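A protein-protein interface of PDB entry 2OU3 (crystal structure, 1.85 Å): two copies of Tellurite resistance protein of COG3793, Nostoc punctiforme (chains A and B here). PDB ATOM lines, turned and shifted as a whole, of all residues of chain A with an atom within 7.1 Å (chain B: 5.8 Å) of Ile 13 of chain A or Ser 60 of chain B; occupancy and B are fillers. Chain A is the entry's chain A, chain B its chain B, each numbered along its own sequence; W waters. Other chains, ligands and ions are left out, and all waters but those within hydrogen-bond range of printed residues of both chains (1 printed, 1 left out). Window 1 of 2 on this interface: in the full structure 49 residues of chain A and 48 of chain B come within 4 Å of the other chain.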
ATOM      1  N   ILE A   5      11.085   9.039   0.752  1.00  0.00           N
ATOM      2  CA  ILE A   5      11.832  10.081   0.041  1.00  0.00           C
ATOM      3  C   ILE A   5      13.320  10.023   0.403  1.00  0.00           C
ATOM      4  O   ILE A   5      14.167  10.115  -0.479  1.00  0.00           O
ATOM      5  CB  ILE A   5      11.228  11.491   0.245  1.00  0.00           C
ATOM      6  CG1 ILE A   5       9.889  11.591  -0.507  1.00  0.00           C
ATOM      7  CG2 ILE A   5      12.181  12.550  -0.273  1.00  0.00           C
ATOM      8  CD1 ILE A   5       9.042  12.723  -0.061  1.00  0.00           C
ATOM      9  N   LYS A   6      13.637   9.803   1.680  1.00  0.00           N
ATOM     10  CA  LYS A   6      15.013   9.551   2.077  1.00  0.00           C
ATOM     11  C   LYS A   6      15.602   8.366   1.313  1.00  0.00           C
ATOM     12  O   LYS A   6      16.709   8.457   0.778  1.00  0.00           O
ATOM     13  CB  LYS A   6      15.105   9.277   3.576  1.00  0.00           C
ATOM     14  CG  LYS A   6      16.537   9.162   4.100  1.00  0.00           C
ATOM     15  N   LYS A   7      14.872   7.264   1.252  1.00  0.00           N
ATOM     16  CA  LYS A   7      15.329   6.106   0.524  1.00  0.00           C
ATOM     17  C   LYS A   7      15.545   6.407  -0.951  1.00  0.00           C
ATOM     18  O   LYS A   7      16.427   5.857  -1.549  1.00  0.00           O
ATOM     19  CB  LYS A   7      14.377   4.913   0.664  1.00  0.00           C
ATOM     20  CG  LYS A   7      14.479   4.236   2.005  1.00  0.00           C
ATOM     21  CD  LYS A   7      13.330   3.244   2.212  1.00  0.00           C
ATOM     22  CE  LYS A   7      13.603   2.303   3.395  1.00  0.00           C
ATOM     23  NZ  LYS A   7      12.368   1.644   3.909  1.00  0.00           N
ATOM     24  N   LEU A   8      14.721   7.271  -1.539  1.00  0.00           N
ATOM     25  CA  LEU A   8      14.930   7.670  -2.918  1.00  0.00           C
ATOM     26  C   LEU A   8      16.300   8.301  -3.131  1.00  0.00           C
ATOM     27  O   LEU A   8      17.040   7.888  -4.060  1.00  0.00           O
ATOM     28  CB  LEU A   8      13.848   8.666  -3.369  1.00  0.00           C
ATOM     29  CG  LEU A   8      13.829   8.942  -4.871  1.00  0.00           C
ATOM     30  CD1 LEU A   8      13.519   7.687  -5.690  1.00  0.00           C
ATOM     31  CD2 LEU A   8      12.777   9.992  -5.111  1.00  0.00           C
ATOM     32  N   GLY A   9      16.642   9.282  -2.277  1.00  0.00           N
ATOM     33  CA  GLY A   9      17.911   9.976  -2.397  1.00  0.00           C
ATOM     34  C   GLY A   9      19.096   9.081  -2.062  1.00  0.00           C
ATOM     35  O   GLY A   9      20.130   9.096  -2.741  1.00  0.00           O
ATOM     36  N   SER A  10      18.965   8.317  -0.992  1.00  0.00           N
ATOM     37  CA  SER A  10      20.046   7.448  -0.573  1.00  0.00           C
ATOM     38  C   SER A  10      20.330   6.337  -1.589  1.00  0.00           C
ATOM     39  O   SER A  10      21.484   6.037  -1.853  1.00  0.00           O
ATOM     40  CB  SER A  10      19.774   6.890   0.823  1.00  0.00           C
ATOM     41  OG  SER A  10      19.847   7.950   1.765  1.00  0.00           O
ATOM     42  N   SER A  11      19.293   5.720  -2.121  1.00  0.00           N
ATOM     43  CA  SER A  11      19.466   4.689  -3.140  1.00  0.00           C
ATOM     44  C   SER A  11      20.171   5.260  -4.371  1.00  0.00           C
ATOM     45  O   SER A  11      21.046   4.616  -4.958  1.00  0.00           O
ATOM     46  CB  SER A  11      18.105   4.141  -3.590  1.00  0.00           C
ATOM     47  OG  SER A  11      17.430   3.515  -2.535  1.00  0.00           O
ATOM     48  N   TRP A  12      19.757   6.468  -4.770  1.00  0.00           N
ATOM     49  CA  TRP A  12      20.282   7.079  -5.983  1.00  0.00           C
ATOM     50  C   TRP A  12      21.757   7.357  -5.806  1.00  0.00           C
ATOM     51  O   TRP A  12      22.569   6.976  -6.644  1.00  0.00           O
ATOM     52  CB  TRP A  12      19.536   8.384  -6.337  1.00  0.00           C
ATOM     53  CG  TRP A  12      19.963   8.968  -7.670  1.00  0.00           C
ATOM     54  CD1 TRP A  12      19.330   8.806  -8.842  1.00  0.00           C
ATOM     55  CD2 TRP A  12      21.096   9.774  -7.943  1.00  0.00           C
ATOM     56  NE1 TRP A  12      19.989   9.448  -9.842  1.00  0.00           N
ATOM     57  CE2 TRP A  12      21.093  10.039  -9.330  1.00  0.00           C
ATOM     58  CE3 TRP A  12      22.115  10.295  -7.169  1.00  0.00           C
ATOM     59  CZ2 TRP A  12      22.055  10.827  -9.947  1.00  0.00           C
ATOM     60  CZ3 TRP A  12      23.064  11.070  -7.770  1.00  0.00           C
ATOM     61  CH2 TRP A  12      23.054  11.295  -9.155  1.00  0.00           C
ATOM     62  N   ILE A  13      22.121   8.003  -4.699  1.00  0.00           N
ATOM     63  CA  ILE A  13      23.503   8.392  -4.483  1.00  0.00           C
ATOM     64  C   ILE A  13      24.421   7.187  -4.228  1.00  0.00           C
ATOM     65  O   ILE A  13      25.583   7.162  -4.668  1.00  0.00           O
ATOM     66  CB  ILE A  13      23.592   9.459  -3.341  1.00  0.00           C
ATOM     67  CG1 ILE A  13      24.852  10.310  -3.486  1.00  0.00           C
ATOM     68  CG2 ILE A  13      23.491   8.819  -1.951  1.00  0.00           C
ATOM     69  CD1 ILE A  13      25.137  10.772  -4.919  1.00  0.00           C
ATOM     70  N   ILE A  14      23.913   6.187  -3.513  1.00  0.00           N
ATOM     71  CA  ILE A  14      24.679   4.957  -3.299  1.00  0.00           C
ATOM     72  C   ILE A  14      24.908   4.272  -4.632  1.00  0.00           C
ATOM     73  O   ILE A  14      26.037   3.866  -4.955  1.00  0.00           O
ATOM     74  CB  ILE A  14      23.961   4.019  -2.323  1.00  0.00           C
ATOM     75  CG1 ILE A  14      24.145   4.524  -0.917  1.00  0.00           C
ATOM     76  CG2 ILE A  14      24.513   2.609  -2.465  1.00  0.00           C
ATOM     77  CD1 ILE A  14      25.626   4.398  -0.382  1.00  0.00           C
ATOM     78  N   ASN A  15      23.863   4.200  -5.452  1.00  0.00           N
ATOM     79  CA  ASN A  15      24.043   3.637  -6.803  1.00  0.00           C
ATOM     80  C   ASN A  15      25.017   4.472  -7.666  1.00  0.00           C
ATOM     81  O   ASN A  15      25.843   3.926  -8.418  1.00  0.00           O
ATOM     82  CB  ASN A  15      22.710   3.441  -7.506  1.00  0.00           C
ATOM     83  CG  ASN A  15      22.870   2.839  -8.872  1.00  0.00           C
ATOM     84  OD1 ASN A  15      22.944   3.562  -9.880  1.00  0.00           O
ATOM     85  ND2 ASN A  15      22.993   1.522  -8.923  1.00  0.00           N
ATOM     86  N   TRP A  16      24.914   5.795  -7.554  1.00  0.00           N
ATOM     87  CA  TRP A  16      25.739   6.674  -8.323  1.00  0.00           C
ATOM     88  C   TRP A  16      27.238   6.417  -8.055  1.00  0.00           C
ATOM     89  O   TRP A  16      28.029   6.257  -8.992  1.00  0.00           O
ATOM     90  CB  TRP A  16      25.390   8.146  -8.066  1.00  0.00           C
ATOM     91  CG  TRP A  16      26.295   9.080  -8.799  1.00  0.00           C
ATOM     92  CD1 TRP A  16      27.391   9.758  -8.276  1.00  0.00           C
ATOM     93  CD2 TRP A  16      26.274   9.392 -10.194  1.00  0.00           C
ATOM     94  NE1 TRP A  16      28.000  10.483  -9.264  1.00  0.00           N
ATOM     95  CE2 TRP A  16      27.346  10.273 -10.446  1.00  0.00           C
ATOM     96  CE3 TRP A  16      25.454   9.018 -11.261  1.00  0.00           C
ATOM     97  CZ2 TRP A  16      27.610  10.770 -11.720  1.00  0.00           C
ATOM     98  CZ3 TRP A  16      25.709   9.521 -12.508  1.00  0.00           C
ATOM     99  CH2 TRP A  16      26.761  10.410 -12.726  1.00  0.00           C
ATOM    100  N   PHE A  17      27.630   6.394  -6.790  1.00  0.00           N
ATOM    101  CA  PHE A  17      29.052   6.302  -6.473  1.00  0.00           C
ATOM    102  C   PHE A  17      29.573   4.867  -6.466  1.00  0.00           C
ATOM    103  O   PHE A  17      30.754   4.638  -6.736  1.00  0.00           O
ATOM    104  CB  PHE A  17      29.323   6.925  -5.109  1.00  0.00           C
ATOM    105  CG  PHE A  17      29.351   8.424  -5.136  1.00  0.00           C
ATOM    106  CD1 PHE A  17      30.329   9.093  -5.848  1.00  0.00           C
ATOM    107  CD2 PHE A  17      28.415   9.167  -4.437  1.00  0.00           C
ATOM    108  CE1 PHE A  17      30.383  10.481  -5.856  1.00  0.00           C
ATOM    109  CE2 PHE A  17      28.467  10.577  -4.448  1.00  0.00           C
ATOM    110  CZ  PHE A  17      29.442  11.214  -5.161  1.00  0.00           C
ATOM    111  N   PHE A  18      28.739   3.920  -6.070  1.00  0.00           N
ATOM    112  CA  PHE A  18      29.246   2.553  -5.841  1.00  0.00           C
ATOM    113  C   PHE A  18      28.647   1.473  -6.738  1.00  0.00           C
ATOM    114  O   PHE A  18      29.171   0.351  -6.754  1.00  0.00           O
ATOM    115  CB  PHE A  18      29.101   2.168  -4.375  1.00  0.00           C
ATOM    116  CG  PHE A  18      29.680   3.194  -3.439  1.00  0.00           C
ATOM    117  CD1 PHE A  18      31.044   3.362  -3.350  1.00  0.00           C
ATOM    118  CD2 PHE A  18      28.844   4.090  -2.771  1.00  0.00           C
ATOM    119  CE1 PHE A  18      31.585   4.345  -2.542  1.00  0.00           C
ATOM    120  CE2 PHE A  18      29.366   5.076  -1.922  1.00  0.00           C
ATOM    121  CZ  PHE A  18      30.734   5.223  -1.836  1.00  0.00           C
ATOM    122  N   GLY A  19      27.573   1.789  -7.466  1.00  0.00           N
ATOM    123  CA  GLY A  19      26.911   0.825  -8.347  1.00  0.00           C
ATOM    124  C   GLY A  19      25.931  -0.112  -7.660  1.00  0.00           C
ATOM    125  O   GLY A  19      25.355  -1.024  -8.296  1.00  0.00           O
ATOM    126  N   PHE A  57      31.417  13.152   2.696  1.00  0.00           N
ATOM    127  CA  PHE A  57      31.134  12.120   1.706  1.00  0.00           C
ATOM    128  C   PHE A  57      30.205  11.100   2.352  1.00  0.00           C
ATOM    129  O   PHE A  57      29.155  10.802   1.822  1.00  0.00           O
ATOM    130  CB  PHE A  57      32.466  11.521   1.266  1.00  0.00           C
ATOM    131  CG  PHE A  57      32.374  10.446   0.236  1.00  0.00           C
ATOM    132  CD1 PHE A  57      31.462  10.509  -0.806  1.00  0.00           C
ATOM    133  CD2 PHE A  57      33.291   9.398   0.283  1.00  0.00           C
ATOM    134  CE1 PHE A  57      31.426   9.519  -1.775  1.00  0.00           C
ATOM    135  CE2 PHE A  57      33.250   8.389  -0.683  1.00  0.00           C
ATOM    136  CZ  PHE A  57      32.331   8.451  -1.692  1.00  0.00           C
ATOM    137  N   SER A  60      26.630  12.435   2.990  1.00  0.00           N
ATOM    138  CA  SER A  60      25.844  12.600   1.775  1.00  0.00           C
ATOM    139  C   SER A  60      25.036  11.370   1.482  1.00  0.00           C
ATOM    140  O   SER A  60      24.041  11.487   0.800  1.00  0.00           O
ATOM    141  CB  SER A  60      26.706  12.936   0.556  1.00  0.00           C
ATOM    142  OG  SER A  60      27.414  11.816   0.101  1.00  0.00           O
ATOM    143  N   TRP A  61      25.462  10.183   1.924  1.00  0.00           N
ATOM    144  CA  TRP A  61      24.696   8.951   1.627  1.00  0.00           C
ATOM    145  C   TRP A  61      23.424   8.844   2.457  1.00  0.00           C
ATOM    146  O   TRP A  61      22.632   7.918   2.278  1.00  0.00           O
ATOM    147  CB  TRP A  61      25.478   7.667   1.871  1.00  0.00           C
ATOM    148  CG  TRP A  61      26.888   7.726   1.393  1.00  0.00           C
ATOM    149  CD1 TRP A  61      27.354   8.440   0.340  1.00  0.00           C
ATOM    150  CD2 TRP A  61      28.018   7.060   1.964  1.00  0.00           C
ATOM    151  NE1 TRP A  61      28.712   8.268   0.219  1.00  0.00           N
ATOM    152  CE2 TRP A  61      29.139   7.410   1.194  1.00  0.00           C
ATOM    153  CE3 TRP A  61      28.190   6.176   3.044  1.00  0.00           C
ATOM    154  CZ2 TRP A  61      30.421   6.938   1.486  1.00  0.00           C
ATOM    155  CZ3 TRP A  61      29.447   5.717   3.326  1.00  0.00           C
ATOM    156  CH2 TRP A  61      30.552   6.099   2.553  1.00  0.00           C
ATOM    157  N   GLY A  62      23.240   9.751   3.387  1.00  0.00           N
ATOM    158  CA  GLY A  62      22.041   9.757   4.244  1.00  0.00           C
ATOM    159  C   GLY A  62      22.083   8.777   5.405  1.00  0.00           C
ATOM    160  O   GLY A  62      21.034   8.410   5.975  1.00  0.00           O
ATOM    161  N   ILE B  13      27.667  17.251  -1.170  1.00  0.00           N
ATOM    162  CA  ILE B  13      27.149  16.748  -2.429  1.00  0.00           C
ATOM    163  C   ILE B  13      26.822  17.911  -3.402  1.00  0.00           C
ATOM    164  O   ILE B  13      27.015  17.784  -4.601  1.00  0.00           O
ATOM    165  CB  ILE B  13      25.935  15.840  -2.198  1.00  0.00           C
ATOM    166  CG1 ILE B  13      25.629  14.958  -3.404  1.00  0.00           C
ATOM    167  CG2 ILE B  13      24.706  16.636  -1.709  1.00  0.00           C
ATOM    168  CD1 ILE B  13      26.848  14.177  -3.965  1.00  0.00           C
ATOM    169  N   PHE B  17      28.726  18.053  -7.152  1.00  0.00           N
ATOM    170  CA  PHE B  17      28.116  18.088  -8.474  1.00  0.00           C
ATOM    171  C   PHE B  17      28.177  19.449  -9.147  1.00  0.00           C
ATOM    172  O   PHE B  17      28.238  19.492 -10.349  1.00  0.00           O
ATOM    173  CB  PHE B  17      26.639  17.650  -8.420  1.00  0.00           C
ATOM    174  CG  PHE B  17      26.455  16.166  -8.278  1.00  0.00           C
ATOM    175  CD1 PHE B  17      26.949  15.298  -9.235  1.00  0.00           C
ATOM    176  CD2 PHE B  17      25.815  15.630  -7.173  1.00  0.00           C
ATOM    177  CE1 PHE B  17      26.770  13.903  -9.128  1.00  0.00           C
ATOM    178  CE2 PHE B  17      25.624  14.226  -7.058  1.00  0.00           C
ATOM    179  CZ  PHE B  17      26.109  13.377  -8.040  1.00  0.00           C
ATOM    180  N   LEU B  55      14.249  12.710  -9.931  1.00  0.00           N
ATOM    181  CA  LEU B  55      13.789  12.859  -8.539  1.00  0.00           C
ATOM    182  C   LEU B  55      14.803  12.329  -7.538  1.00  0.00           C
ATOM    183  O   LEU B  55      15.022  12.904  -6.446  1.00  0.00           O
ATOM    184  CB  LEU B  55      12.501  12.078  -8.341  1.00  0.00           C
ATOM    185  CG  LEU B  55      11.201  12.513  -9.049  1.00  0.00           C
ATOM    186  CD1 LEU B  55      10.120  11.482  -8.887  1.00  0.00           C
ATOM    187  CD2 LEU B  55      10.713  13.796  -8.534  1.00  0.00           C
ATOM    188  N   GLY B  56      15.438  11.234  -7.910  1.00  0.00           N
ATOM    189  CA  GLY B  56      16.480  10.634  -7.069  1.00  0.00           C
ATOM    190  C   GLY B  56      17.713  11.500  -7.018  1.00  0.00           C
ATOM    191  O   GLY B  56      18.305  11.636  -5.967  1.00  0.00           O
ATOM    192  N   PHE B  57      18.093  12.085  -8.158  1.00  0.00           N
ATOM    193  CA  PHE B  57      19.200  13.077  -8.232  1.00  0.00           C
ATOM    194  C   PHE B  57      18.926  14.258  -7.293  1.00  0.00           C
ATOM    195  O   PHE B  57      19.770  14.669  -6.480  1.00  0.00           O
ATOM    196  CB  PHE B  57      19.355  13.530  -9.707  1.00  0.00           C
ATOM    197  CG  PHE B  57      20.488  14.509  -9.970  1.00  0.00           C
ATOM    198  CD1 PHE B  57      21.713  14.386  -9.337  1.00  0.00           C
ATOM    199  CD2 PHE B  57      20.315  15.530 -10.904  1.00  0.00           C
ATOM    200  CE1 PHE B  57      22.769  15.263  -9.634  1.00  0.00           C
ATOM    201  CE2 PHE B  57      21.357  16.417 -11.190  1.00  0.00           C
ATOM    202  CZ  PHE B  57      22.571  16.288 -10.550  1.00  0.00           C
ATOM    203  N   CYS B  58      17.731  14.821  -7.406  1.00  0.00           N
ATOM    204  CA  CYS B  58      17.321  15.942  -6.574  1.00  0.00           C
ATOM    205  C   CYS B  58      17.286  15.558  -5.081  1.00  0.00           C
ATOM    206  O   CYS B  58      17.844  16.252  -4.238  1.00  0.00           O
ATOM    207  CB  CYS B  58      15.965  16.474  -7.071  1.00  0.00           C
ATOM    208  SG  CYS B  58      15.315  17.880  -6.094  1.00  0.00           S
ATOM    209  N   ALA B  59      16.669  14.421  -4.780  1.00  0.00           N
ATOM    210  CA  ALA B  59      16.571  13.943  -3.411  1.00  0.00           C
ATOM    211  C   ALA B  59      17.975  13.729  -2.800  1.00  0.00           C
ATOM    212  O   ALA B  59      18.180  13.992  -1.643  1.00  0.00           O
ATOM    213  CB  ALA B  59      15.775  12.681  -3.377  1.00  0.00           C
ATOM    214  N   SER B  60      18.947  13.311  -3.613  1.00  0.00           N
ATOM    215  CA  SER B  60      20.309  13.097  -3.114  1.00  0.00           C
ATOM    216  C   SER B  60      20.939  14.377  -2.583  1.00  0.00           C
ATOM    217  O   SER B  60      21.872  14.279  -1.809  1.00  0.00           O
ATOM    218  CB  SER B  60      21.257  12.506  -4.176  1.00  0.00           C
ATOM    219  OG  SER B  60      21.759  13.493  -5.043  1.00  0.00           O
ATOM    220  N   TRP B  61      20.454  15.565  -2.976  1.00  0.00           N
ATOM    221  CA  TRP B  61      21.037  16.797  -2.435  1.00  0.00           C
ATOM    222  C   TRP B  61      20.596  17.125  -1.009  1.00  0.00           C
ATOM    223  O   TRP B  61      21.147  18.058  -0.400  1.00  0.00           O
ATOM    224  CB  TRP B  61      20.748  17.988  -3.328  1.00  0.00           C
ATOM    225  CG  TRP B  61      20.866  17.757  -4.789  1.00  0.00           C
ATOM    226  CD1 TRP B  61      21.753  16.947  -5.437  1.00  0.00           C
ATOM    227  CD2 TRP B  61      20.119  18.424  -5.782  1.00  0.00           C
ATOM    228  NE1 TRP B  61      21.570  17.045  -6.789  1.00  0.00           N
ATOM    229  CE2 TRP B  61      20.563  17.946  -7.029  1.00  0.00           C
ATOM    230  CE3 TRP B  61      19.063  19.359  -5.742  1.00  0.00           C
ATOM    231  CZ2 TRP B  61      19.985  18.340  -8.219  1.00  0.00           C
ATOM    232  CZ3 TRP B  61      18.522  19.780  -6.940  1.00  0.00           C
ATOM    233  CH2 TRP B  61      18.983  19.266  -8.158  1.00  0.00           C
ATOM    234  N   GLY B  62      19.645  16.365  -0.477  1.00  0.00           N
ATOM    235  CA  GLY B  62      19.130  16.583   0.874  1.00  0.00           C
ATOM    236  C   GLY B  62      18.067  17.668   0.974  1.00  0.00           C
ATOM    237  O   GLY B  62      17.826  18.207   2.057  1.00  0.00           O
ATOM    238  N   VAL B  63      17.423  17.968  -0.152  1.00  0.00           N
ATOM    239  CA  VAL B  63      16.303  18.910  -0.213  1.00  0.00           C
ATOM    240  C   VAL B  63      15.207  18.474   0.772  1.00  0.00           C
ATOM    241  O   VAL B  63      15.110  17.305   1.130  1.00  0.00           O
ATOM    242  CB  VAL B  63      15.731  19.074  -1.674  1.00  0.00           C
ATOM    243  CG1 VAL B  63      16.815  19.586  -2.621  1.00  0.00           C
ATOM    244  CG2 VAL B  63      15.106  17.775  -2.173  1.00  0.00           C
HETATM  245  O   HOH W   1      22.778  13.989   0.687  1.00  0.00           O
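O of Phe 57 of chain B is in hydrogen-bond range of OG of Ser 60 of chain B (2.7 Å). NE1 of Trp 61 of chain B lies within hydrogen-bond range of O of Phe 57 of chain B (3.0 Å).
Among the printed residues, pairs that only touch across the chains: Trp 12 of chain A with Phe 57 of chain B, Trp 12 of chain A with Gly 56 of chain B, Gly 9 of chain A with Ala 59 of chain B, Trp 16 of chain A with Phe 17 of chain B, Gly 9 of chain A with Ser 60 of chain B, Trp 12 of chain A with Ser 60 of chain B, Trp 12 of chain A with Phe 17 of chain B, Leu 8 of chain A with Gly 56 of chain B, Leu 8 of chain A with Leu 55 of chain B, Ile 13 of chain A with Ile 13 of chain B, Ile 13 of chain A with Ser 60 of chain B, Gly 9 of chain A with Gly 56 of chain B and Phe 17 of chain A with Ile 13 of chain B.
Of the printed residues of chain B, Ile 13 of chain A touches Ile 13 and Ser 60. Of the printed residues of chain A, Ser 60 of chain B touches Gly 9 (3.7 Å), Trp 12 (3.8 Å) and Ile 13 (3.9 Å). Printed residues of chain B within 4 Å of Gly 9 of chain A: Gly 56, Ala 59 and Ser 60. Of the printed residues of chain A, Ile 13 of chain B touches Ile 13 and Phe 17. Trp 61 of chain B touches none of the printed residues of chain A. Ser 60 of chain A touches none of the printed residues of chain B. The nearest printed residue of chain B that does not touch Ile 13 of chain A is Phe 17 of chain B (4.1 Å). The nearest printed residue of chain A that does not touch Ser 60 of chain B is Ser 60 of chain A (4.4 Å). The nearest printed residue of chain B that does not touch Phe 17 of chain A is Phe 17 of chain B (4.9 Å).
Printed residues of chain B that touch a printed residue of chain A: Ile 13, Phe 17, Leu 55, Gly 56, Phe 57, Ala 59 and Ser 60. Hydrophobic or aromatic side chains of chain B within 4 Å of the printed part of chain A: Ile 13, Phe 17, Leu 55, Phe 57 and Ala 59.
Ile 13 of chain B touches its own counterpart, Ile 13 of chain A. Ile 13 of chain A touches Ser 60 of chain B, but with the chains exchanged Ser 60 of chain A does not touch Ile 13 of chain B (4.1 Å). Phe 17 of chain A touches Ile 13 of chain B, but with the chains exchanged Ile 13 of chain A does not touch Phe 17 of chain B (4.1 Å). 6 positions are printed for both chains.
Water W1 bridges O of Ser 60 of chain B and O of Ser 60 of chain A.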
